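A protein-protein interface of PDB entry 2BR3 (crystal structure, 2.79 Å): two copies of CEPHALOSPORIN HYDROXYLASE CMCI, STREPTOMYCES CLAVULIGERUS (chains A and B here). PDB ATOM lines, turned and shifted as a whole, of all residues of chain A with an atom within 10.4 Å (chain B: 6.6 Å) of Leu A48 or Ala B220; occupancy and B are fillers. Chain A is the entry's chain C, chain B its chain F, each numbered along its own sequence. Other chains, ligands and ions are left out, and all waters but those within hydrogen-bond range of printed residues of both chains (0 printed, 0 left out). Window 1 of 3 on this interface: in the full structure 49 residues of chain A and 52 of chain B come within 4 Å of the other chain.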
ATOM      1  N   PRO A  27       6.601 -32.598  -2.528  1.00  0.00           N
ATOM      2  CA  PRO A  27       7.841 -32.648  -1.759  1.00  0.00           C
ATOM      3  C   PRO A  27       7.752 -33.678  -0.634  1.00  0.00           C
ATOM      4  O   PRO A  27       6.662 -34.036  -0.186  1.00  0.00           O
ATOM      5  CB  PRO A  27       7.972 -31.225  -1.198  1.00  0.00           C
ATOM      6  CG  PRO A  27       7.021 -30.408  -1.996  1.00  0.00           C
ATOM      7  CD  PRO A  27       5.893 -31.318  -2.352  1.00  0.00           C
ATOM      8  N   VAL A  28       8.909 -34.169  -0.213  1.00  0.00           N
ATOM      9  CA  VAL A  28       9.013 -34.979   0.994  1.00  0.00           C
ATOM     10  C   VAL A  28      10.113 -34.410   1.859  1.00  0.00           C
ATOM     11  O   VAL A  28      11.060 -33.783   1.362  1.00  0.00           O
ATOM     12  CB  VAL A  28       9.334 -36.453   0.699  1.00  0.00           C
ATOM     13  CG1 VAL A  28       8.063 -37.201   0.309  1.00  0.00           C
ATOM     14  CG2 VAL A  28      10.428 -36.577  -0.377  1.00  0.00           C
ATOM     15  N   LEU A  29       9.978 -34.626   3.160  1.00  0.00           N
ATOM     16  CA  LEU A  29      10.990 -34.201   4.105  1.00  0.00           C
ATOM     17  C   LEU A  29      11.998 -35.341   4.291  1.00  0.00           C
ATOM     18  O   LEU A  29      11.671 -36.518   4.084  1.00  0.00           O
ATOM     19  CB  LEU A  29      10.334 -33.808   5.432  1.00  0.00           C
ATOM     20  CG  LEU A  29       9.334 -32.632   5.457  1.00  0.00           C
ATOM     21  CD1 LEU A  29       9.650 -31.542   4.438  1.00  0.00           C
ATOM     22  CD2 LEU A  29       7.902 -33.113   5.266  1.00  0.00           C
ATOM     23  N   THR A  30      13.233 -34.980   4.635  1.00  0.00           N
ATOM     24  CA  THR A  30      14.263 -35.955   4.994  1.00  0.00           C
ATOM     25  C   THR A  30      14.682 -35.766   6.460  1.00  0.00           C
ATOM     26  O   THR A  30      14.688 -36.719   7.245  1.00  0.00           O
ATOM     27  CB  THR A  30      15.497 -35.844   4.040  1.00  0.00           C
ATOM     28  OG1 THR A  30      16.198 -34.606   4.253  1.00  0.00           O
ATOM     29  CG2 THR A  30      15.071 -35.792   2.559  1.00  0.00           C
ATOM     30  N   ASP A  31      14.990 -34.525   6.829  1.00  0.00           N
ATOM     31  CA  ASP A  31      15.550 -34.224   8.151  1.00  0.00           C
ATOM     32  C   ASP A  31      14.521 -33.902   9.248  1.00  0.00           C
ATOM     33  O   ASP A  31      14.904 -33.516  10.351  1.00  0.00           O
ATOM     34  CB  ASP A  31      16.609 -33.109   8.045  1.00  0.00           C
ATOM     35  CG  ASP A  31      16.025 -31.768   7.645  1.00  0.00           C
ATOM     36  OD1 ASP A  31      14.913 -31.720   7.088  1.00  0.00           O
ATOM     37  OD2 ASP A  31      16.628 -30.699   7.839  1.00  0.00           O
ATOM     38  N   ARG A  32      13.230 -34.064   8.968  1.00  0.00           N
ATOM     39  CA  ARG A  32      12.218 -33.891  10.017  1.00  0.00           C
ATOM     40  C   ARG A  32      10.960 -34.713   9.826  1.00  0.00           C
ATOM     41  O   ARG A  32      10.590 -35.057   8.700  1.00  0.00           O
ATOM     42  CB  ARG A  32      11.791 -32.423  10.163  1.00  0.00           C
ATOM     43  CG  ARG A  32      12.374 -31.453   9.138  1.00  0.00           C
ATOM     44  CD  ARG A  32      11.369 -30.787   8.194  1.00  0.00           C
ATOM     45  NE  ARG A  32      11.476 -29.335   8.247  1.00  0.00           N
ATOM     46  CZ  ARG A  32      12.565 -28.642   7.951  1.00  0.00           C
ATOM     47  NH1 ARG A  32      13.672 -29.244   7.554  1.00  0.00           N
ATOM     48  NH2 ARG A  32      12.537 -27.325   8.047  1.00  0.00           N
ATOM     49  N   PRO A  33      10.288 -35.016  10.933  1.00  0.00           N
ATOM     50  CA  PRO A  33       8.926 -35.556  10.856  1.00  0.00           C
ATOM     51  C   PRO A  33       7.946 -34.532  10.280  1.00  0.00           C
ATOM     52  O   PRO A  33       8.123 -33.326  10.468  1.00  0.00           O
ATOM     53  CB  PRO A  33       8.583 -35.894  12.318  1.00  0.00           C
ATOM     54  CG  PRO A  33       9.528 -35.098  13.141  1.00  0.00           C
ATOM     55  CD  PRO A  33      10.762 -34.900  12.325  1.00  0.00           C
ATOM     56  N   ARG A  34       6.932 -35.026   9.577  1.00  0.00           N
ATOM     57  CA  ARG A  34       5.852 -34.186   9.080  1.00  0.00           C
ATOM     58  C   ARG A  34       4.965 -33.663  10.212  1.00  0.00           C
ATOM     59  O   ARG A  34       4.456 -32.559  10.137  1.00  0.00           O
ATOM     60  CB  ARG A  34       5.007 -34.943   8.054  1.00  0.00           C
ATOM     61  CG  ARG A  34       4.410 -34.030   7.003  1.00  0.00           C
ATOM     62  CD  ARG A  34       3.311 -34.651   6.153  1.00  0.00           C
ATOM     63  NE  ARG A  34       2.247 -33.683   5.876  1.00  0.00           N
ATOM     64  CZ  ARG A  34       1.534 -33.621   4.755  1.00  0.00           C
ATOM     65  NH1 ARG A  34       1.727 -34.485   3.765  1.00  0.00           N
ATOM     66  NH2 ARG A  34       0.609 -32.683   4.620  1.00  0.00           N
ATOM     67  N   ALA A  44      11.273 -26.356  16.519  1.00  0.00           N
ATOM     68  CA  ALA A  44      11.085 -26.825  15.155  1.00  0.00           C
ATOM     69  C   ALA A  44      11.888 -25.969  14.165  1.00  0.00           C
ATOM     70  O   ALA A  44      12.018 -24.759  14.356  1.00  0.00           O
ATOM     71  CB  ALA A  44       9.597 -26.831  14.795  1.00  0.00           C
ATOM     72  N   PRO A  45      12.426 -26.592  13.114  1.00  0.00           N
ATOM     73  CA  PRO A  45      13.220 -25.860  12.125  1.00  0.00           C
ATOM     74  C   PRO A  45      12.362 -24.861  11.373  1.00  0.00           C
ATOM     75  O   PRO A  45      11.160 -25.083  11.222  1.00  0.00           O
ATOM     76  CB  PRO A  45      13.728 -26.966  11.190  1.00  0.00           C
ATOM     77  CG  PRO A  45      12.780 -28.085  11.350  1.00  0.00           C
ATOM     78  CD  PRO A  45      12.315 -28.025  12.772  1.00  0.00           C
ATOM     79  N   ARG A  46      12.993 -23.789  10.897  1.00  0.00           N
ATOM     80  CA  ARG A  46      12.294 -22.635  10.328  1.00  0.00           C
ATOM     81  C   ARG A  46      12.341 -22.562   8.816  1.00  0.00           C
ATOM     82  O   ARG A  46      11.593 -21.807   8.218  1.00  0.00           O
ATOM     83  CB  ARG A  46      12.896 -21.356  10.897  1.00  0.00           C
ATOM     84  CG  ARG A  46      12.617 -21.171  12.369  1.00  0.00           C
ATOM     85  CD  ARG A  46      11.217 -20.702  12.646  1.00  0.00           C
ATOM     86  NE  ARG A  46      11.052 -19.314  12.226  1.00  0.00           N
ATOM     87  CZ  ARG A  46      11.471 -18.264  12.916  1.00  0.00           C
ATOM     88  NH1 ARG A  46      12.084 -18.422  14.086  1.00  0.00           N
ATOM     89  NH2 ARG A  46      11.275 -17.045  12.438  1.00  0.00           N
ATOM     90  N   ASP A  47      13.228 -23.330   8.199  1.00  0.00           N
ATOM     91  CA  ASP A  47      13.368 -23.327   6.745  1.00  0.00           C
ATOM     92  C   ASP A  47      12.325 -24.238   6.098  1.00  0.00           C
ATOM     93  O   ASP A  47      11.582 -24.938   6.775  1.00  0.00           O
ATOM     94  CB  ASP A  47      14.797 -23.718   6.334  1.00  0.00           C
ATOM     95  CG  ASP A  47      15.140 -25.158   6.676  1.00  0.00           C
ATOM     96  OD1 ASP A  47      15.307 -25.982   5.751  1.00  0.00           O
ATOM     97  OD2 ASP A  47      15.266 -25.559   7.848  1.00  0.00           O
ATOM     98  N   LEU A  48      12.287 -24.220   4.775  1.00  0.00           N
ATOM     99  CA  LEU A  48      11.244 -24.890   4.008  1.00  0.00           C
ATOM    100  C   LEU A  48      11.200 -26.409   4.186  1.00  0.00           C
ATOM    101  O   LEU A  48      10.117 -26.993   4.287  1.00  0.00           O
ATOM    102  CB  LEU A  48      11.432 -24.567   2.527  1.00  0.00           C
ATOM    103  CG  LEU A  48      10.198 -24.674   1.649  1.00  0.00           C
ATOM    104  CD1 LEU A  48       9.030 -23.918   2.274  1.00  0.00           C
ATOM    105  CD2 LEU A  48      10.522 -24.160   0.253  1.00  0.00           C
ATOM    106  N   GLY A  49      12.366 -27.048   4.202  1.00  0.00           N
ATOM    107  CA  GLY A  49      12.445 -28.494   4.340  1.00  0.00           C
ATOM    108  C   GLY A  49      12.697 -29.236   3.037  1.00  0.00           C
ATOM    109  O   GLY A  49      13.166 -30.367   3.050  1.00  0.00           O
ATOM    110  N   TYR A  50      12.387 -28.601   1.911  1.00  0.00           N
ATOM    111  CA  TYR A  50      12.677 -29.170   0.594  1.00  0.00           C
ATOM    112  C   TYR A  50      13.263 -28.105  -0.353  1.00  0.00           C
ATOM    113  O   TYR A  50      13.283 -26.909  -0.029  1.00  0.00           O
ATOM    114  CB  TYR A  50      11.397 -29.778   0.002  1.00  0.00           C
ATOM    115  CG  TYR A  50      10.217 -28.833   0.014  1.00  0.00           C
ATOM    116  CD1 TYR A  50       9.991 -27.964  -1.038  1.00  0.00           C
ATOM    117  CD2 TYR A  50       9.335 -28.800   1.087  1.00  0.00           C
ATOM    118  CE1 TYR A  50       8.915 -27.093  -1.030  1.00  0.00           C
ATOM    119  CE2 TYR A  50       8.258 -27.924   1.106  1.00  0.00           C
ATOM    120  CZ  TYR A  50       8.055 -27.079   0.041  1.00  0.00           C
ATOM    121  OH  TYR A  50       7.000 -26.214   0.041  1.00  0.00           O
ATOM    122  N   SER A  51      13.749 -28.539  -1.515  1.00  0.00           N
ATOM    123  CA  SER A  51      14.246 -27.604  -2.527  1.00  0.00           C
ATOM    124  C   SER A  51      13.141 -26.686  -3.079  1.00  0.00           C
ATOM    125  O   SER A  51      12.098 -27.156  -3.560  1.00  0.00           O
ATOM    126  CB  SER A  51      14.903 -28.354  -3.685  1.00  0.00           C
ATOM    127  OG  SER A  51      15.251 -27.463  -4.737  1.00  0.00           O
ATOM    128  N   ASP A  52      13.394 -25.379  -3.027  1.00  0.00           N
ATOM    129  CA  ASP A  52      12.458 -24.381  -3.542  1.00  0.00           C
ATOM    130  C   ASP A  52      12.703 -23.994  -5.016  1.00  0.00           C
ATOM    131  O   ASP A  52      12.437 -22.845  -5.405  1.00  0.00           O
ATOM    132  CB  ASP A  52      12.482 -23.127  -2.652  1.00  0.00           C
ATOM    133  CG  ASP A  52      13.740 -22.285  -2.833  1.00  0.00           C
ATOM    134  OD1 ASP A  52      13.702 -21.103  -2.441  1.00  0.00           O
ATOM    135  OD2 ASP A  52      14.803 -22.715  -3.344  1.00  0.00           O
ATOM    136  N   PHE A  53      13.175 -24.941  -5.835  1.00  0.00           N
ATOM    137  CA  PHE A  53      13.494 -24.635  -7.236  1.00  0.00           C
ATOM    138  C   PHE A  53      12.226 -24.304  -8.039  1.00  0.00           C
ATOM    139  O   PHE A  53      12.046 -23.164  -8.488  1.00  0.00           O
ATOM    140  CB  PHE A  53      14.300 -25.761  -7.927  1.00  0.00           C
ATOM    141  CG  PHE A  53      14.114 -25.799  -9.436  1.00  0.00           C
ATOM    142  CD1 PHE A  53      13.744 -26.970 -10.078  1.00  0.00           C
ATOM    143  CD2 PHE A  53      14.269 -24.641 -10.207  1.00  0.00           C
ATOM    144  CE1 PHE A  53      13.547 -26.989 -11.456  1.00  0.00           C
ATOM    145  CE2 PHE A  53      14.062 -24.662 -11.586  1.00  0.00           C
ATOM    146  CZ  PHE A  53      13.702 -25.832 -12.205  1.00  0.00           C
ATOM    147  N   SER A  54      11.370 -25.293  -8.252  1.00  0.00           N
ATOM    148  CA  SER A  54      10.127 -25.055  -8.969  1.00  0.00           C
ATOM    149  C   SER A  54       9.078 -25.960  -8.362  1.00  0.00           C
ATOM    150  O   SER A  54       8.591 -26.866  -9.022  1.00  0.00           O
ATOM    151  CB  SER A  54      10.309 -25.330 -10.473  1.00  0.00           C
ATOM    152  OG  SER A  54       9.113 -25.114 -11.215  1.00  0.00           O
ATOM    153  N   PRO A  55       8.721 -25.703  -7.106  1.00  0.00           N
ATOM    154  CA  PRO A  55       7.814 -26.575  -6.363  1.00  0.00           C
ATOM    155  C   PRO A  55       6.339 -26.232  -6.563  1.00  0.00           C
ATOM    156  O   PRO A  55       5.543 -26.643  -5.744  1.00  0.00           O
ATOM    157  CB  PRO A  55       8.204 -26.284  -4.917  1.00  0.00           C
ATOM    158  CG  PRO A  55       8.477 -24.830  -4.941  1.00  0.00           C
ATOM    159  CD  PRO A  55       9.113 -24.538  -6.292  1.00  0.00           C
ATOM    160  N   TYR A  56       5.970 -25.511  -7.611  1.00  0.00           N
ATOM    161  CA  TYR A  56       4.587 -25.058  -7.769  1.00  0.00           C
ATOM    162  C   TYR A  56       3.751 -26.023  -8.629  1.00  0.00           C
ATOM    163  O   TYR A  56       4.292 -26.865  -9.341  1.00  0.00           O
ATOM    164  CB  TYR A  56       4.583 -23.605  -8.289  1.00  0.00           C
ATOM    165  CG  TYR A  56       5.289 -22.682  -7.305  1.00  0.00           C
ATOM    166  CD1 TYR A  56       6.511 -22.068  -7.619  1.00  0.00           C
ATOM    167  CD2 TYR A  56       4.761 -22.480  -6.023  1.00  0.00           C
ATOM    168  CE1 TYR A  56       7.165 -21.257  -6.688  1.00  0.00           C
ATOM    169  CE2 TYR A  56       5.405 -21.671  -5.089  1.00  0.00           C
ATOM    170  CZ  TYR A  56       6.605 -21.064  -5.422  1.00  0.00           C
ATOM    171  OH  TYR A  56       7.213 -20.263  -4.475  1.00  0.00           O
ATOM    172  N   PRO A  67       3.986 -18.085  -8.017  1.00  0.00           N
ATOM    173  CA  PRO A  67       2.810 -17.344  -7.537  1.00  0.00           C
ATOM    174  C   PRO A  67       2.738 -15.870  -7.919  1.00  0.00           C
ATOM    175  O   PRO A  67       1.670 -15.393  -8.250  1.00  0.00           O
ATOM    176  CB  PRO A  67       2.931 -17.475  -6.020  1.00  0.00           C
ATOM    177  CG  PRO A  67       3.575 -18.796  -5.827  1.00  0.00           C
ATOM    178  CD  PRO A  67       4.570 -18.909  -6.941  1.00  0.00           C
ATOM    179  N   ASP A  68       3.847 -15.153  -7.862  1.00  0.00           N
ATOM    180  CA  ASP A  68       3.829 -13.734  -8.176  1.00  0.00           C
ATOM    181  C   ASP A  68       3.538 -13.498  -9.644  1.00  0.00           C
ATOM    182  O   ASP A  68       2.855 -12.540  -9.994  1.00  0.00           O
ATOM    183  CB  ASP A  68       5.163 -13.101  -7.806  1.00  0.00           C
ATOM    184  CG  ASP A  68       5.404 -13.100  -6.310  1.00  0.00           C
ATOM    185  OD1 ASP A  68       6.411 -13.702  -5.875  1.00  0.00           O
ATOM    186  OD2 ASP A  68       4.627 -12.535  -5.502  1.00  0.00           O
ATOM    187  N   ASP B  68       1.722 -16.506  -2.081  1.00  0.00           N
ATOM    188  CA  ASP B  68       2.421 -17.619  -1.445  1.00  0.00           C
ATOM    189  C   ASP B  68       1.479 -18.448  -0.580  1.00  0.00           C
ATOM    190  O   ASP B  68       1.570 -19.676  -0.552  1.00  0.00           O
ATOM    191  CB  ASP B  68       3.597 -17.096  -0.636  1.00  0.00           C
ATOM    192  CG  ASP B  68       4.670 -16.494  -1.522  1.00  0.00           C
ATOM    193  OD1 ASP B  68       5.094 -15.352  -1.243  1.00  0.00           O
ATOM    194  OD2 ASP B  68       5.136 -17.088  -2.525  1.00  0.00           O
ATOM    195  N   THR B  69       0.583 -17.753   0.113  1.00  0.00           N
ATOM    196  CA  THR B  69      -0.506 -18.374   0.854  1.00  0.00           C
ATOM    197  C   THR B  69      -1.495 -19.111  -0.075  1.00  0.00           C
ATOM    198  O   THR B  69      -2.000 -20.177   0.262  1.00  0.00           O
ATOM    199  CB  THR B  69      -1.246 -17.290   1.671  1.00  0.00           C
ATOM    200  OG1 THR B  69      -0.357 -16.726   2.638  1.00  0.00           O
ATOM    201  CG2 THR B  69      -2.382 -17.891   2.504  1.00  0.00           C
ATOM    202  N   ALA B  71      -0.678 -20.480  -2.863  1.00  0.00           N
ATOM    203  CA  ALA B  71      -0.004 -21.684  -3.335  1.00  0.00           C
ATOM    204  C   ALA B  71      -0.088 -22.794  -2.290  1.00  0.00           C
ATOM    205  O   ALA B  71      -0.263 -23.956  -2.634  1.00  0.00           O
ATOM    206  CB  ALA B  71       1.433 -21.391  -3.684  1.00  0.00           C
ATOM    207  N   VAL B  72       0.022 -22.434  -1.015  1.00  0.00           N
ATOM    208  CA  VAL B  72      -0.036 -23.423   0.054  1.00  0.00           C
ATOM    209  C   VAL B  72      -1.450 -24.025   0.162  1.00  0.00           C
ATOM    210  O   VAL B  72      -1.612 -25.240   0.175  1.00  0.00           O
ATOM    211  CB  VAL B  72       0.391 -22.822   1.394  1.00  0.00           C
ATOM    212  CG1 VAL B  72       0.123 -23.804   2.544  1.00  0.00           C
ATOM    213  CG2 VAL B  72       1.855 -22.433   1.354  1.00  0.00           C
ATOM    214  N   MET B 215       4.543 -29.814   9.063  1.00  0.00           N
ATOM    215  CA  MET B 215       5.802 -29.198   8.623  1.00  0.00           C
ATOM    216  C   MET B 215       5.934 -29.028   7.114  1.00  0.00           C
ATOM    217  O   MET B 215       6.732 -28.240   6.646  1.00  0.00           O
ATOM    218  CB  MET B 215       6.992 -30.008   9.155  1.00  0.00           C
ATOM    219  CG  MET B 215       7.113 -29.988  10.666  1.00  0.00           C
ATOM    220  SD  MET B 215       7.222 -28.299  11.299  1.00  0.00           S
ATOM    221  CE  MET B 215       8.967 -27.910  10.992  1.00  0.00           C
ATOM    222  N   LEU B 216       5.149 -29.774   6.362  1.00  0.00           N
ATOM    223  CA  LEU B 216       5.115 -29.641   4.909  1.00  0.00           C
ATOM    224  C   LEU B 216       4.547 -28.293   4.451  1.00  0.00           C
ATOM    225  O   LEU B 216       4.925 -27.794   3.393  1.00  0.00           O
ATOM    226  CB  LEU B 216       4.277 -30.785   4.294  1.00  0.00           C
ATOM    227  CG  LEU B 216       4.457 -30.987   2.789  1.00  0.00           C
ATOM    228  CD1 LEU B 216       5.800 -31.630   2.511  1.00  0.00           C
ATOM    229  CD2 LEU B 216       3.328 -31.797   2.218  1.00  0.00           C
ATOM    230  N   TYR B 217       3.619 -27.733   5.223  1.00  0.00           N
ATOM    231  CA  TYR B 217       2.978 -26.473   4.869  1.00  0.00           C
ATOM    232  C   TYR B 217       3.321 -25.301   5.805  1.00  0.00           C
ATOM    233  O   TYR B 217       3.108 -24.140   5.442  1.00  0.00           O
ATOM    234  CB  TYR B 217       1.458 -26.661   4.823  1.00  0.00           C
ATOM    235  CG  TYR B 217       0.979 -27.684   3.812  1.00  0.00           C
ATOM    236  CD1 TYR B 217       0.083 -28.693   4.171  1.00  0.00           C
ATOM    237  CD2 TYR B 217       1.412 -27.641   2.494  1.00  0.00           C
ATOM    238  CE1 TYR B 217      -0.356 -29.640   3.232  1.00  0.00           C
ATOM    239  CE2 TYR B 217       0.986 -28.580   1.557  1.00  0.00           C
ATOM    240  CZ  TYR B 217       0.106 -29.573   1.927  1.00  0.00           C
ATOM    241  OH  TYR B 217      -0.301 -30.478   0.972  1.00  0.00           O
ATOM    242  N   ALA B 218       3.872 -25.579   6.985  1.00  0.00           N
ATOM    243  CA  ALA B 218       3.945 -24.557   8.038  1.00  0.00           C
ATOM    244  C   ALA B 218       5.113 -23.591   7.927  1.00  0.00           C
ATOM    245  O   ALA B 218       5.237 -22.700   8.749  1.00  0.00           O
ATOM    246  CB  ALA B 218       3.960 -25.210   9.396  1.00  0.00           C
ATOM    247  N   ASN B 219       5.973 -23.764   6.934  1.00  0.00           N
ATOM    248  CA  ASN B 219       7.074 -22.831   6.695  1.00  0.00           C
ATOM    249  C   ASN B 219       7.094 -22.356   5.242  1.00  0.00           C
ATOM    250  O   ASN B 219       8.140 -21.980   4.732  1.00  0.00           O
ATOM    251  CB  ASN B 219       8.407 -23.497   7.068  1.00  0.00           C
ATOM    252  CG  ASN B 219       8.600 -23.608   8.572  1.00  0.00           C
ATOM    253  OD1 ASN B 219       8.096 -22.775   9.328  1.00  0.00           O
ATOM    254  ND2 ASN B 219       9.332 -24.624   9.016  1.00  0.00           N
ATOM    255  N   ALA B 220       5.930 -22.355   4.594  1.00  0.00           N
ATOM    256  CA  ALA B 220       5.849 -22.158   3.151  1.00  0.00           C
ATOM    257  C   ALA B 220       5.198 -20.831   2.778  1.00  0.00           C
ATOM    258  O   ALA B 220       5.067 -20.508   1.597  1.00  0.00           O
ATOM    259  CB  ALA B 220       5.090 -23.319   2.507  1.00  0.00           C
ATOM    260  N   SER B 221       4.772 -20.068   3.771  1.00  0.00           N
ATOM    261  CA  SER B 221       4.335 -18.693   3.531  1.00  0.00           C
ATOM    262  C   SER B 221       4.405 -17.896   4.827  1.00  0.00           C
ATOM    263  O   SER B 221       4.259 -18.444   5.920  1.00  0.00           O
ATOM    264  CB  SER B 221       2.922 -18.648   2.944  1.00  0.00           C
ATOM    265  OG  SER B 221       1.933 -18.508   3.957  1.00  0.00           O
ATOM    266  N   SER B 222       4.627 -16.598   4.708  1.00  0.00           N
ATOM    267  CA  SER B 222       4.806 -15.771   5.882  1.00  0.00           C
ATOM    268  C   SER B 222       3.492 -15.595   6.651  1.00  0.00           C
ATOM    269  O   SER B 222       3.505 -15.469   7.846  1.00  0.00           O
ATOM    270  CB  SER B 222       5.471 -14.435   5.511  1.00  0.00           C
ATOM    271  OG  SER B 222       4.566 -13.535   4.924  1.00  0.00           O
ATOM    272  N   LEU B 224       1.138 -17.901   7.062  1.00  0.00           N
ATOM    273  CA  LEU B 224       0.831 -19.158   7.739  1.00  0.00           C
ATOM    274  C   LEU B 224       1.980 -19.636   8.632  1.00  0.00           C
ATOM    275  O   LEU B 224       1.879 -20.663   9.290  1.00  0.00           O
ATOM    276  CB  LEU B 224       0.544 -20.224   6.693  1.00  0.00           C
ATOM    277  CG  LEU B 224      -0.568 -19.923   5.689  1.00  0.00           C
ATOM    278  CD1 LEU B 224      -0.585 -20.998   4.620  1.00  0.00           C
ATOM    279  CD2 LEU B 224      -1.921 -19.823   6.373  1.00  0.00           C
ATOM    280  N   ASP B 225       3.075 -18.884   8.634  1.00  0.00           N
ATOM    281  CA  ASP B 225       4.282 -19.229   9.371  1.00  0.00           C
ATOM    282  C   ASP B 225       3.973 -19.817  10.748  1.00  0.00           C
ATOM    283  O   ASP B 225       3.370 -19.157  11.592  1.00  0.00           O
ATOM    284  CB  ASP B 225       5.166 -17.983   9.515  1.00  0.00           C
ATOM    285  CG  ASP B 225       6.496 -18.275  10.193  1.00  0.00           C
ATOM    286  OD1 ASP B 225       6.954 -19.437  10.192  1.00  0.00           O
ATOM    287  OD2 ASP B 225       7.172 -17.394  10.751  1.00  0.00           O
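The backbone carbonyl oxygen of Arg A34 is in hydrogen-bond range of the backbone NH of Met B215 (2.9 Å).
The backbone carbonyl oxygen (O) of Asp A47 lies within hydrogen-bond range of the side-chain amide nitrogen (ND2) of Asn B219, 3.2 Å away.
The backbone carbonyl oxygen of Pro A45 is in hydrogen-bond range of the side-chain amide nitrogen of Asn B219 (2.9 Å).
The backbone NH of Gly A49 sits close to the side-chain carboxylate of Asp A47, 3.5 Å away.
The side-chain carboxylate (OD1) of Asp A31 lies within salt-bridge range of the guanidinium group (NH1) of Arg A32, 2.8 Å away.
OD2 of Asp A47 is in salt-bridge range of NH2 of Arg A32, 3.3 Å away.
Leu B216 touches Pro A27 (CD1 to O, 3.7 Å).
Leu B216 touches Leu A29 (CD1 to CD2, 3.8 Å).
Arg A32 touches Met B215.
Pro A33 touches Met B215 (O to CG, 3.5 Å).
NH2 of Arg A34 touches CE1 of Tyr B217 (3.5 Å).
Pro A45 touches Met B215.
Arg A46 touches Asn B219 (O to CG, 3.5 Å).
Leu A48 touches Asn B219 (CD1 to O, 3.3 Å).
Leu A48 touches Ala B220.
CB of Ala B71 touches CG of Pro A67 (3.99 Å).
Of chain B, only Asn B219 (3.3 Å) and Ala B220 (3.7 Å) come within 4 Å of Leu A48.
Ala B220 touches one residue of chain A.
No residue of chain A comes within 4 Å of Ala B218.
Asn B219 touches four residues of chain A.
Of the printed residues of chain A, Ala B71 touches Pro A67 (3.99 Å).
Printed residues of chain A within 4 Å of Leu B216: Pro A27 (3.7 Å), Leu A29 (3.8 Å) and Arg A34 (3.5 Å).
Pro A55 touches none of the printed residues of chain B.
Asp B225 touches none of the printed residues of chain A.
The nearest residue of chain A that does not touch Ala B220 is Tyr A50 (4.3 Å).
Among the printed residues, no Asp or Glu carboxylate lies within 4 Å of a Lys or Arg side-chain nitrogen of the other chain.
1 position is printed for both chains.
Of the 14 pairs that touch across the chains among the printed residues, none has its exchanged pair printed and touching as well.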
